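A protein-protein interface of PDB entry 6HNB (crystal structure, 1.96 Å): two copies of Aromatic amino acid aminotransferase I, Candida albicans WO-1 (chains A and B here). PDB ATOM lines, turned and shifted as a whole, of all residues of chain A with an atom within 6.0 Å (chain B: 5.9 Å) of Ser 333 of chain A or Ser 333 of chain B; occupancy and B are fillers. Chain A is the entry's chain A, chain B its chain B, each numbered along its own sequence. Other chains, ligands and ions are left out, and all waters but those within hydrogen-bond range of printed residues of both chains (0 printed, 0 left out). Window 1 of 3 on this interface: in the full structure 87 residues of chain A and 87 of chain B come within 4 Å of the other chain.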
ATOM      1  N   SER A 102       8.993  -0.954  36.113  1.00  0.00           N
ATOM      2  CA  SER A 102       8.536  -0.822  34.707  1.00  0.00           C
ATOM      3  C   SER A 102       9.386   0.253  34.000  1.00  0.00           C
ATOM      4  O   SER A 102       9.574   0.110  32.787  1.00  0.00           O
ATOM      5  CB  SER A 102       7.050  -0.589  34.596  1.00  0.00           C
ATOM      6  OG  SER A 102       6.653   0.551  35.326  1.00  0.00           O
ATOM      7  N   LEU A 111       7.889  -7.718  30.660  1.00  0.00           N
ATOM      8  CA  LEU A 111       7.586  -7.620  32.121  1.00  0.00           C
ATOM      9  C   LEU A 111       6.680  -8.799  32.500  1.00  0.00           C
ATOM     10  O   LEU A 111       5.750  -9.107  31.763  1.00  0.00           O
ATOM     11  CB  LEU A 111       6.980  -6.238  32.389  1.00  0.00           C
ATOM     12  CG  LEU A 111       7.972  -5.074  32.234  1.00  0.00           C
ATOM     13  CD1 LEU A 111       7.261  -3.728  32.101  1.00  0.00           C
ATOM     14  CD2 LEU A 111       8.967  -5.044  33.387  1.00  0.00           C
ATOM     15  N   VAL A 139       7.273  -4.225  19.803  1.00  0.00           N
ATOM     16  CA  VAL A 139       6.794  -2.824  19.841  1.00  0.00           C
ATOM     17  C   VAL A 139       5.806  -2.618  18.699  1.00  0.00           C
ATOM     18  O   VAL A 139       5.650  -1.460  18.282  1.00  0.00           O
ATOM     19  CB  VAL A 139       7.975  -1.837  19.864  1.00  0.00           C
ATOM     20  CG1 VAL A 139       8.777  -2.041  21.145  1.00  0.00           C
ATOM     21  CG2 VAL A 139       8.856  -1.942  18.627  1.00  0.00           C
ATOM     22  N   GLY A 305      -0.649   3.960  19.336  1.00  0.00           N
ATOM     23  CA  GLY A 305       0.435   4.623  20.077  1.00  0.00           C
ATOM     24  C   GLY A 305       0.912   3.834  21.262  1.00  0.00           C
ATOM     25  O   GLY A 305       1.924   4.223  21.826  1.00  0.00           O
ATOM     26  N   LEU A 306       0.223   2.749  21.637  1.00  0.00           N
ATOM     27  CA  LEU A 306       0.807   1.789  22.616  1.00  0.00           C
ATOM     28  C   LEU A 306       2.196   1.342  22.139  1.00  0.00           C
ATOM     29  O   LEU A 306       3.089   1.217  22.987  1.00  0.00           O
ATOM     30  CB  LEU A 306      -0.134   0.595  22.835  1.00  0.00           C
ATOM     31  CG  LEU A 306      -1.125   0.767  23.982  1.00  0.00           C
ATOM     32  CD1 LEU A 306      -2.182  -0.316  23.949  1.00  0.00           C
ATOM     33  CD2 LEU A 306      -0.416   0.762  25.325  1.00  0.00           C
ATOM     34  N   ARG A 307       2.384   1.124  20.838  1.00  0.00           N
ATOM     35  CA  ARG A 307       3.625   0.496  20.301  1.00  0.00           C
ATOM     36  C   ARG A 307       3.919  -0.755  21.152  1.00  0.00           C
ATOM     37  O   ARG A 307       5.031  -0.884  21.720  1.00  0.00           O
ATOM     38  CB  ARG A 307       4.811   1.475  20.282  1.00  0.00           C
ATOM     39  CG  ARG A 307       4.689   2.659  19.326  1.00  0.00           C
ATOM     40  CD  ARG A 307       3.801   2.488  18.090  1.00  0.00           C
ATOM     41  NE  ARG A 307       4.239   1.486  17.121  1.00  0.00           N
ATOM     42  CZ  ARG A 307       3.452   0.771  16.292  1.00  0.00           C
ATOM     43  NH1 ARG A 307       2.124   0.903  16.283  1.00  0.00           N
ATOM     44  NH2 ARG A 307       4.024  -0.111  15.478  1.00  0.00           N
ATOM     45  N   LEU A 308       2.929  -1.631  21.259  1.00  0.00           N
ATOM     46  CA  LEU A 308       3.024  -2.857  22.057  1.00  0.00           C
ATOM     47  C   LEU A 308       2.291  -3.971  21.316  1.00  0.00           C
ATOM     48  O   LEU A 308       1.092  -3.834  21.005  1.00  0.00           O
ATOM     49  CB  LEU A 308       2.403  -2.598  23.425  1.00  0.00           C
ATOM     50  CG  LEU A 308       2.580  -3.689  24.468  1.00  0.00           C
ATOM     51  CD1 LEU A 308       4.053  -3.986  24.766  1.00  0.00           C
ATOM     52  CD2 LEU A 308       1.849  -3.279  25.734  1.00  0.00           C
ATOM     53  N   ASN A 331      13.310  -2.944  24.504  1.00  0.00           N
ATOM     54  CA  ASN A 331      12.016  -3.259  25.174  1.00  0.00           C
ATOM     55  C   ASN A 331      10.987  -2.214  24.762  1.00  0.00           C
ATOM     56  O   ASN A 331      11.345  -1.108  24.354  1.00  0.00           O
ATOM     57  CB  ASN A 331      12.089  -3.251  26.710  1.00  0.00           C
ATOM     58  CG  ASN A 331      12.200  -4.633  27.325  1.00  0.00           C
ATOM     59  OD1 ASN A 331      11.487  -5.570  26.930  1.00  0.00           O
ATOM     60  ND2 ASN A 331      13.078  -4.764  28.308  1.00  0.00           N
ATOM     61  N   PRO A 332       9.677  -2.537  24.843  1.00  0.00           N
ATOM     62  CA  PRO A 332       8.644  -1.529  24.646  1.00  0.00           C
ATOM     63  C   PRO A 332       8.715  -0.530  25.810  1.00  0.00           C
ATOM     64  O   PRO A 332       9.274  -0.842  26.868  1.00  0.00           O
ATOM     65  CB  PRO A 332       7.317  -2.324  24.637  1.00  0.00           C
ATOM     66  CG  PRO A 332       7.719  -3.795  24.600  1.00  0.00           C
ATOM     67  CD  PRO A 332       9.118  -3.853  25.184  1.00  0.00           C
ATOM     68  N   SER A 333       8.205   0.670  25.581  1.00  0.00           N
ATOM     69  CA  SER A 333       7.941   1.676  26.632  1.00  0.00           C
ATOM     70  C   SER A 333       7.377   0.975  27.874  1.00  0.00           C
ATOM     71  O   SER A 333       6.362   0.229  27.756  1.00  0.00           O
ATOM     72  CB  SER A 333       7.016   2.705  26.107  1.00  0.00           C
ATOM     73  OG  SER A 333       6.529   3.547  27.124  1.00  0.00           O
ATOM     74  N   GLY A 334       7.984   1.234  29.038  1.00  0.00           N
ATOM     75  CA  GLY A 334       7.461   0.784  30.345  1.00  0.00           C
ATOM     76  C   GLY A 334       6.148   1.474  30.682  1.00  0.00           C
ATOM     77  O   GLY A 334       5.317   0.845  31.408  1.00  0.00           O
ATOM     78  N   PHE A 335       5.920   2.702  30.183  1.00  0.00           N
ATOM     79  CA  PHE A 335       4.604   3.358  30.353  1.00  0.00           C
ATOM     80  C   PHE A 335       3.574   2.527  29.587  1.00  0.00           C
ATOM     81  O   PHE A 335       2.523   2.164  30.174  1.00  0.00           O
ATOM     82  CB  PHE A 335       4.594   4.815  29.901  1.00  0.00           C
ATOM     83  CG  PHE A 335       5.403   5.739  30.772  1.00  0.00           C
ATOM     84  CD1 PHE A 335       4.978   6.066  32.056  1.00  0.00           C
ATOM     85  CD2 PHE A 335       6.575   6.301  30.305  1.00  0.00           C
ATOM     86  CE1 PHE A 335       5.722   6.924  32.856  1.00  0.00           C
ATOM     87  CE2 PHE A 335       7.302   7.184  31.094  1.00  0.00           C
ATOM     88  CZ  PHE A 335       6.878   7.494  32.370  1.00  0.00           C
ATOM     89  N   SER A 336       3.866   2.223  28.326  1.00  0.00           N
ATOM     90  CA  SER A 336       2.949   1.419  27.471  1.00  0.00           C
ATOM     91  C   SER A 336       2.662   0.062  28.140  1.00  0.00           C
ATOM     92  O   SER A 336       1.477  -0.317  28.278  1.00  0.00           O
ATOM     93  CB  SER A 336       3.488   1.248  26.074  1.00  0.00           C
ATOM     94  OG  SER A 336       3.240   2.404  25.287  1.00  0.00           O
ATOM     95  N   GLU A 337       3.691  -0.670  28.535  1.00  0.00           N
ATOM     96  CA  GLU A 337       3.495  -2.029  29.082  1.00  0.00           C
ATOM     97  C   GLU A 337       2.798  -1.929  30.456  1.00  0.00           C
ATOM     98  O   GLU A 337       1.880  -2.713  30.713  1.00  0.00           O
ATOM     99  CB  GLU A 337       4.838  -2.748  29.106  1.00  0.00           C
ATOM    100  CG  GLU A 337       4.690  -4.245  29.086  1.00  0.00           C
ATOM    101  CD  GLU A 337       5.980  -4.999  28.822  1.00  0.00           C
ATOM    102  OE1 GLU A 337       6.944  -4.390  28.312  1.00  0.00           O
ATOM    103  OE2 GLU A 337       5.995  -6.197  29.121  1.00  0.00           O
ATOM    104  N   ALA A 338       3.199  -1.002  31.317  1.00  0.00           N
ATOM    105  CA  ALA A 338       2.624  -0.835  32.671  1.00  0.00           C
ATOM    106  C   ALA A 338       1.154  -0.410  32.574  1.00  0.00           C
ATOM    107  O   ALA A 338       0.328  -1.026  33.263  1.00  0.00           O
ATOM    108  CB  ALA A 338       3.464   0.125  33.499  1.00  0.00           C
ATOM    109  N   SER B 102      -1.554  11.705  19.801  1.00  0.00           N
ATOM    110  CA  SER B 102      -0.305  11.044  20.271  1.00  0.00           C
ATOM    111  C   SER B 102      -0.457   9.502  20.281  1.00  0.00           C
ATOM    112  O   SER B 102       0.582   8.824  20.189  1.00  0.00           O
ATOM    113  CB  SER B 102       0.175  11.602  21.592  1.00  0.00           C
ATOM    114  OG  SER B 102      -0.834  11.554  22.573  1.00  0.00           O
ATOM    115  N   VAL B 139      13.706   5.279  19.677  1.00  0.00           N
ATOM    116  CA  VAL B 139      13.199   4.597  20.896  1.00  0.00           C
ATOM    117  C   VAL B 139      14.391   4.256  21.795  1.00  0.00           C
ATOM    118  O   VAL B 139      14.265   3.339  22.597  1.00  0.00           O
ATOM    119  CB  VAL B 139      12.336   3.391  20.481  1.00  0.00           C
ATOM    120  CG1 VAL B 139      11.248   3.848  19.508  1.00  0.00           C
ATOM    121  CG2 VAL B 139      13.148   2.280  19.852  1.00  0.00           C
ATOM    122  N   GLY B 305      12.885   3.335  30.845  1.00  0.00           N
ATOM    123  CA  GLY B 305      11.580   2.802  30.407  1.00  0.00           C
ATOM    124  C   GLY B 305      10.834   3.767  29.502  1.00  0.00           C
ATOM    125  O   GLY B 305       9.756   3.393  28.974  1.00  0.00           O
ATOM    126  N   LEU B 306      11.326   4.991  29.366  1.00  0.00           N
ATOM    127  CA  LEU B 306      10.762   5.936  28.379  1.00  0.00           C
ATOM    128  C   LEU B 306      10.914   5.309  26.989  1.00  0.00           C
ATOM    129  O   LEU B 306       9.969   5.450  26.185  1.00  0.00           O
ATOM    130  CB  LEU B 306      11.436   7.307  28.477  1.00  0.00           C
ATOM    131  CG  LEU B 306      10.690   8.350  29.306  1.00  0.00           C
ATOM    132  CD1 LEU B 306      11.534   9.606  29.481  1.00  0.00           C
ATOM    133  CD2 LEU B 306       9.358   8.710  28.658  1.00  0.00           C
ATOM    134  N   ARG B 307      12.029   4.626  26.709  1.00  0.00           N
ATOM    135  CA  ARG B 307      12.300   4.115  25.340  1.00  0.00           C
ATOM    136  C   ARG B 307      12.126   5.271  24.356  1.00  0.00           C
ATOM    137  O   ARG B 307      11.372   5.141  23.354  1.00  0.00           O
ATOM    138  CB  ARG B 307      11.389   2.931  24.982  1.00  0.00           C
ATOM    139  CG  ARG B 307      11.660   1.683  25.805  1.00  0.00           C
ATOM    140  CD  ARG B 307      13.022   1.069  25.470  1.00  0.00           C
ATOM    141  NE  ARG B 307      14.102   1.580  26.309  1.00  0.00           N
ATOM    142  CZ  ARG B 307      15.395   1.728  25.969  1.00  0.00           C
ATOM    143  NH1 ARG B 307      15.855   1.438  24.756  1.00  0.00           N
ATOM    144  NH2 ARG B 307      16.229   2.197  26.880  1.00  0.00           N
ATOM    145  N   ASN B 331       7.731   4.267  15.390  1.00  0.00           N
ATOM    146  CA  ASN B 331       7.622   5.491  16.221  1.00  0.00           C
ATOM    147  C   ASN B 331       7.743   5.088  17.679  1.00  0.00           C
ATOM    148  O   ASN B 331       7.340   3.979  18.022  1.00  0.00           O
ATOM    149  CB  ASN B 331       6.278   6.203  16.034  1.00  0.00           C
ATOM    150  CG  ASN B 331       6.379   7.443  15.174  1.00  0.00           C
ATOM    151  OD1 ASN B 331       7.295   8.259  15.343  1.00  0.00           O
ATOM    152  ND2 ASN B 331       5.447   7.580  14.242  1.00  0.00           N
ATOM    153  N   PRO B 332       8.191   5.991  18.581  1.00  0.00           N
ATOM    154  CA  PRO B 332       8.179   5.704  20.013  1.00  0.00           C
ATOM    155  C   PRO B 332       6.740   5.584  20.518  1.00  0.00           C
ATOM    156  O   PRO B 332       5.841   6.080  19.835  1.00  0.00           O
ATOM    157  CB  PRO B 332       8.863   6.940  20.634  1.00  0.00           C
ATOM    158  CG  PRO B 332       9.595   7.565  19.465  1.00  0.00           C
ATOM    159  CD  PRO B 332       8.657   7.358  18.303  1.00  0.00           C
ATOM    160  N   SER B 333       6.555   4.951  21.677  1.00  0.00           N
ATOM    161  CA  SER B 333       5.277   4.981  22.431  1.00  0.00           C
ATOM    162  C   SER B 333       4.739   6.424  22.483  1.00  0.00           C
ATOM    163  O   SER B 333       5.477   7.359  22.935  1.00  0.00           O
ATOM    164  CB  SER B 333       5.436   4.429  23.816  1.00  0.00           C
ATOM    165  OG  SER B 333       4.285   4.715  24.621  1.00  0.00           O
ATOM    166  N   GLY B 334       3.476   6.592  22.085  1.00  0.00           N
ATOM    167  CA  GLY B 334       2.739   7.848  22.236  1.00  0.00           C
ATOM    168  C   GLY B 334       2.623   8.240  23.697  1.00  0.00           C
ATOM    169  O   GLY B 334       2.614   9.425  23.985  1.00  0.00           O
ATOM    170  N   PHE B 335       2.501   7.273  24.605  1.00  0.00           N
ATOM    171  CA  PHE B 335       2.487   7.560  26.061  1.00  0.00           C
ATOM    172  C   PHE B 335       3.826   8.161  26.457  1.00  0.00           C
ATOM    173  O   PHE B 335       3.837   9.143  27.208  1.00  0.00           O
ATOM    174  CB  PHE B 335       2.190   6.297  26.867  1.00  0.00           C
ATOM    175  CG  PHE B 335       0.764   5.839  26.750  1.00  0.00           C
ATOM    176  CD1 PHE B 335      -0.264   6.592  27.292  1.00  0.00           C
ATOM    177  CD2 PHE B 335       0.450   4.669  26.084  1.00  0.00           C
ATOM    178  CE1 PHE B 335      -1.578   6.163  27.189  1.00  0.00           C
ATOM    179  CE2 PHE B 335      -0.868   4.245  25.976  1.00  0.00           C
ATOM    180  CZ  PHE B 335      -1.877   4.990  26.543  1.00  0.00           C
ATOM    181  N   SER B 336       4.927   7.527  26.046  1.00  0.00           N
ATOM    182  CA  SER B 336       6.300   8.012  26.349  1.00  0.00           C
ATOM    183  C   SER B 336       6.470   9.421  25.788  1.00  0.00           C
ATOM    184  O   SER B 336       6.847  10.346  26.537  1.00  0.00           O
ATOM    185  CB  SER B 336       7.355   7.080  25.817  1.00  0.00           C
ATOM    186  OG  SER B 336       7.390   5.910  26.625  1.00  0.00           O
ATOM    187  N   GLU B 337       6.208   9.586  24.499  1.00  0.00           N
ATOM    188  CA  GLU B 337       6.440  10.900  23.850  1.00  0.00           C
ATOM    189  C   GLU B 337       5.495  11.963  24.435  1.00  0.00           C
ATOM    190  O   GLU B 337       5.951  13.082  24.662  1.00  0.00           O
ATOM    191  CB  GLU B 337       6.332  10.772  22.341  1.00  0.00           C
ATOM    192  CG  GLU B 337       7.151  11.825  21.657  1.00  0.00           C
ATOM    193  CD  GLU B 337       7.263  11.676  20.159  1.00  0.00           C
ATOM    194  OE1 GLU B 337       7.155  10.514  19.663  1.00  0.00           O
ATOM    195  OE2 GLU B 337       7.434  12.733  19.511  1.00  0.00           O
ATOM    196  N   ALA B 338       4.223  11.654  24.677  1.00  0.00           N
ATOM    197  CA  ALA B 338       3.255  12.645  25.222  1.00  0.00           C
ATOM    198  C   ALA B 338       3.663  13.027  26.647  1.00  0.00           C
ATOM    199  O   ALA B 338       3.566  14.236  27.005  1.00  0.00           O
ATOM    200  CB  ALA B 338       1.850  12.091  25.213  1.00  0.00           C
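Gly 305 of chain A touches Gly 334 of chain B, and with the chains exchanged Gly 334 of chain A touches Gly 305 of chain B. Leu 306 of chain A touches Phe 335 of chain B, and with the chains exchanged Phe 335 of chain A touches Leu 306 of chain B. Arg 307 of chain A touches Ser 333 of chain B, and with the chains exchanged Ser 333 of chain A touches Arg 307 of chain B. Phe 335 of chain A touches Ser 336 of chain B, and with the chains exchanged Ser 336 of chain A touches Phe 335 of chain B. Positions printed for both chains: 102, 139, 305, 306, 307, 331, 332, 333, 334, 335, 336, 337 and 338. Of the 17 pairs that touch across the chains among the printed residues, 17 have their exchanged pair printed and touching as well.
The backbone carbonyl oxygen (O) of Gly 305 of chain A is in hydrogen-bond range of the backbone NH (N) of Gly 334 of chain B (2.8 Å). The side-chain hydroxyl of Ser 336 of chain B is in hydrogen-bond range of the side-chain hydroxyl of Ser 333 of chain A. The backbone carbonyl oxygen of Gly 305 of chain B lies within hydrogen-bond range of the backbone NH of Gly 334 of chain A (2.8 Å). The side-chain hydroxyl (OG) of Ser 336 of chain A sits at hydrogen-bond distance from the side-chain hydroxyl (OG) of Ser 333 of chain B (2.6 Å).
Among the printed residues, merely in contact across the chains: Gly 305 of chain A with Ser 333 of chain B (3.5 Å), Leu 306 of chain A with Phe 335 of chain B (3.6 Å), Arg 307 of chain A with Asn 331 of chain B (3.2 Å), Arg 307 of chain A with Pro 332 of chain B (3.6 Å), Arg 307 of chain A with Ser 333 of chain B (3.8 Å), Asn 331 of chain A with Arg 307 of chain B (3.0 Å), Pro 332 of chain A with Arg 307 of chain B (3.6 Å), Ser 333 of chain A with Gly 305 of chain B (3.4 Å), Ser 333 of chain A with Arg 307 of chain B (3.6 Å), Ser 333 of chain A with Ser 333 of chain B (3.3 Å), Phe 335 of chain A with Leu 306 of chain B (3.5 Å), Phe 335 of chain A with Ser 336 of chain B (3.8 Å) and Ser 336 of chain A with Phe 335 of chain B (3.7 Å).
Along chain A the printed residues that touch a printed residue of chain B span positions 305 to 336. Of the 13 printed residues of chain B, 9 touch a printed residue of chain A. Hydrophobic or aromatic side chains of chain B within 4 Å of the printed part of chain A: Leu 306 and Phe 335. Among the printed residues, 17 pairs touch across the chains.
Of the printed residues of chain B, Leu 306 of chain A touches Phe 335 (3.6 Å). Printed residues of chain B within 4 Å of Ser 333 of chain A: Gly 305 (3.4 Å), Arg 307 (3.6 Å), Ser 333 (3.3 Å) and Ser 336 (2.6 Å). Printed residues of chain B within 4 Å of Ser 336 of chain A: Ser 333 (2.6 Å) and Phe 335 (3.7 Å). Of the printed residues of chain A, Asn 331 of chain B touches Arg 307. Ser 333 of chain B touches just these residues of chain A: Gly 305 (3.5 Å), Arg 307 (3.8 Å), Ser 333 (3.3 Å) and Ser 336 (2.6 Å). The nearest residue of chain B that does not touch Ser 333 of chain A is Leu 306 of chain B (4.03 Å). The nearest residue of chain A that does not touch Ser 333 of chain B is Leu 306 of chain A (4.04 Å). The nearest printed residue of chain B that does not touch Ser 336 of chain A is Gly 334 of chain B (5.3 Å).
OG of Ser 333 of chain B sits at hydrogen-bond distance from N of Phe 335 of chain B (3.1 Å). OG of Ser 333 of chain A sits close to N of Phe 335 of chain A (3.2 Å). OG of Ser 333 of chain B sits at hydrogen-bond distance from N of Ser 336 of chain B, 3.2 Å away. The backbone carbonyl oxygen of Leu 306 of chain B sits at hydrogen-bond distance from the side-chain hydroxyl of Ser 336 of chain B. The backbone NH of Ser 336 of chain A lies within hydrogen-bond range of the side-chain hydroxyl of Ser 333 of chain A, 3.2 Å away. The guanidinium group (NE) of Arg 307 of chain A lies close to the backbone carbonyl oxygen (O) of Val 139 of chain A, 3.5 Å away.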
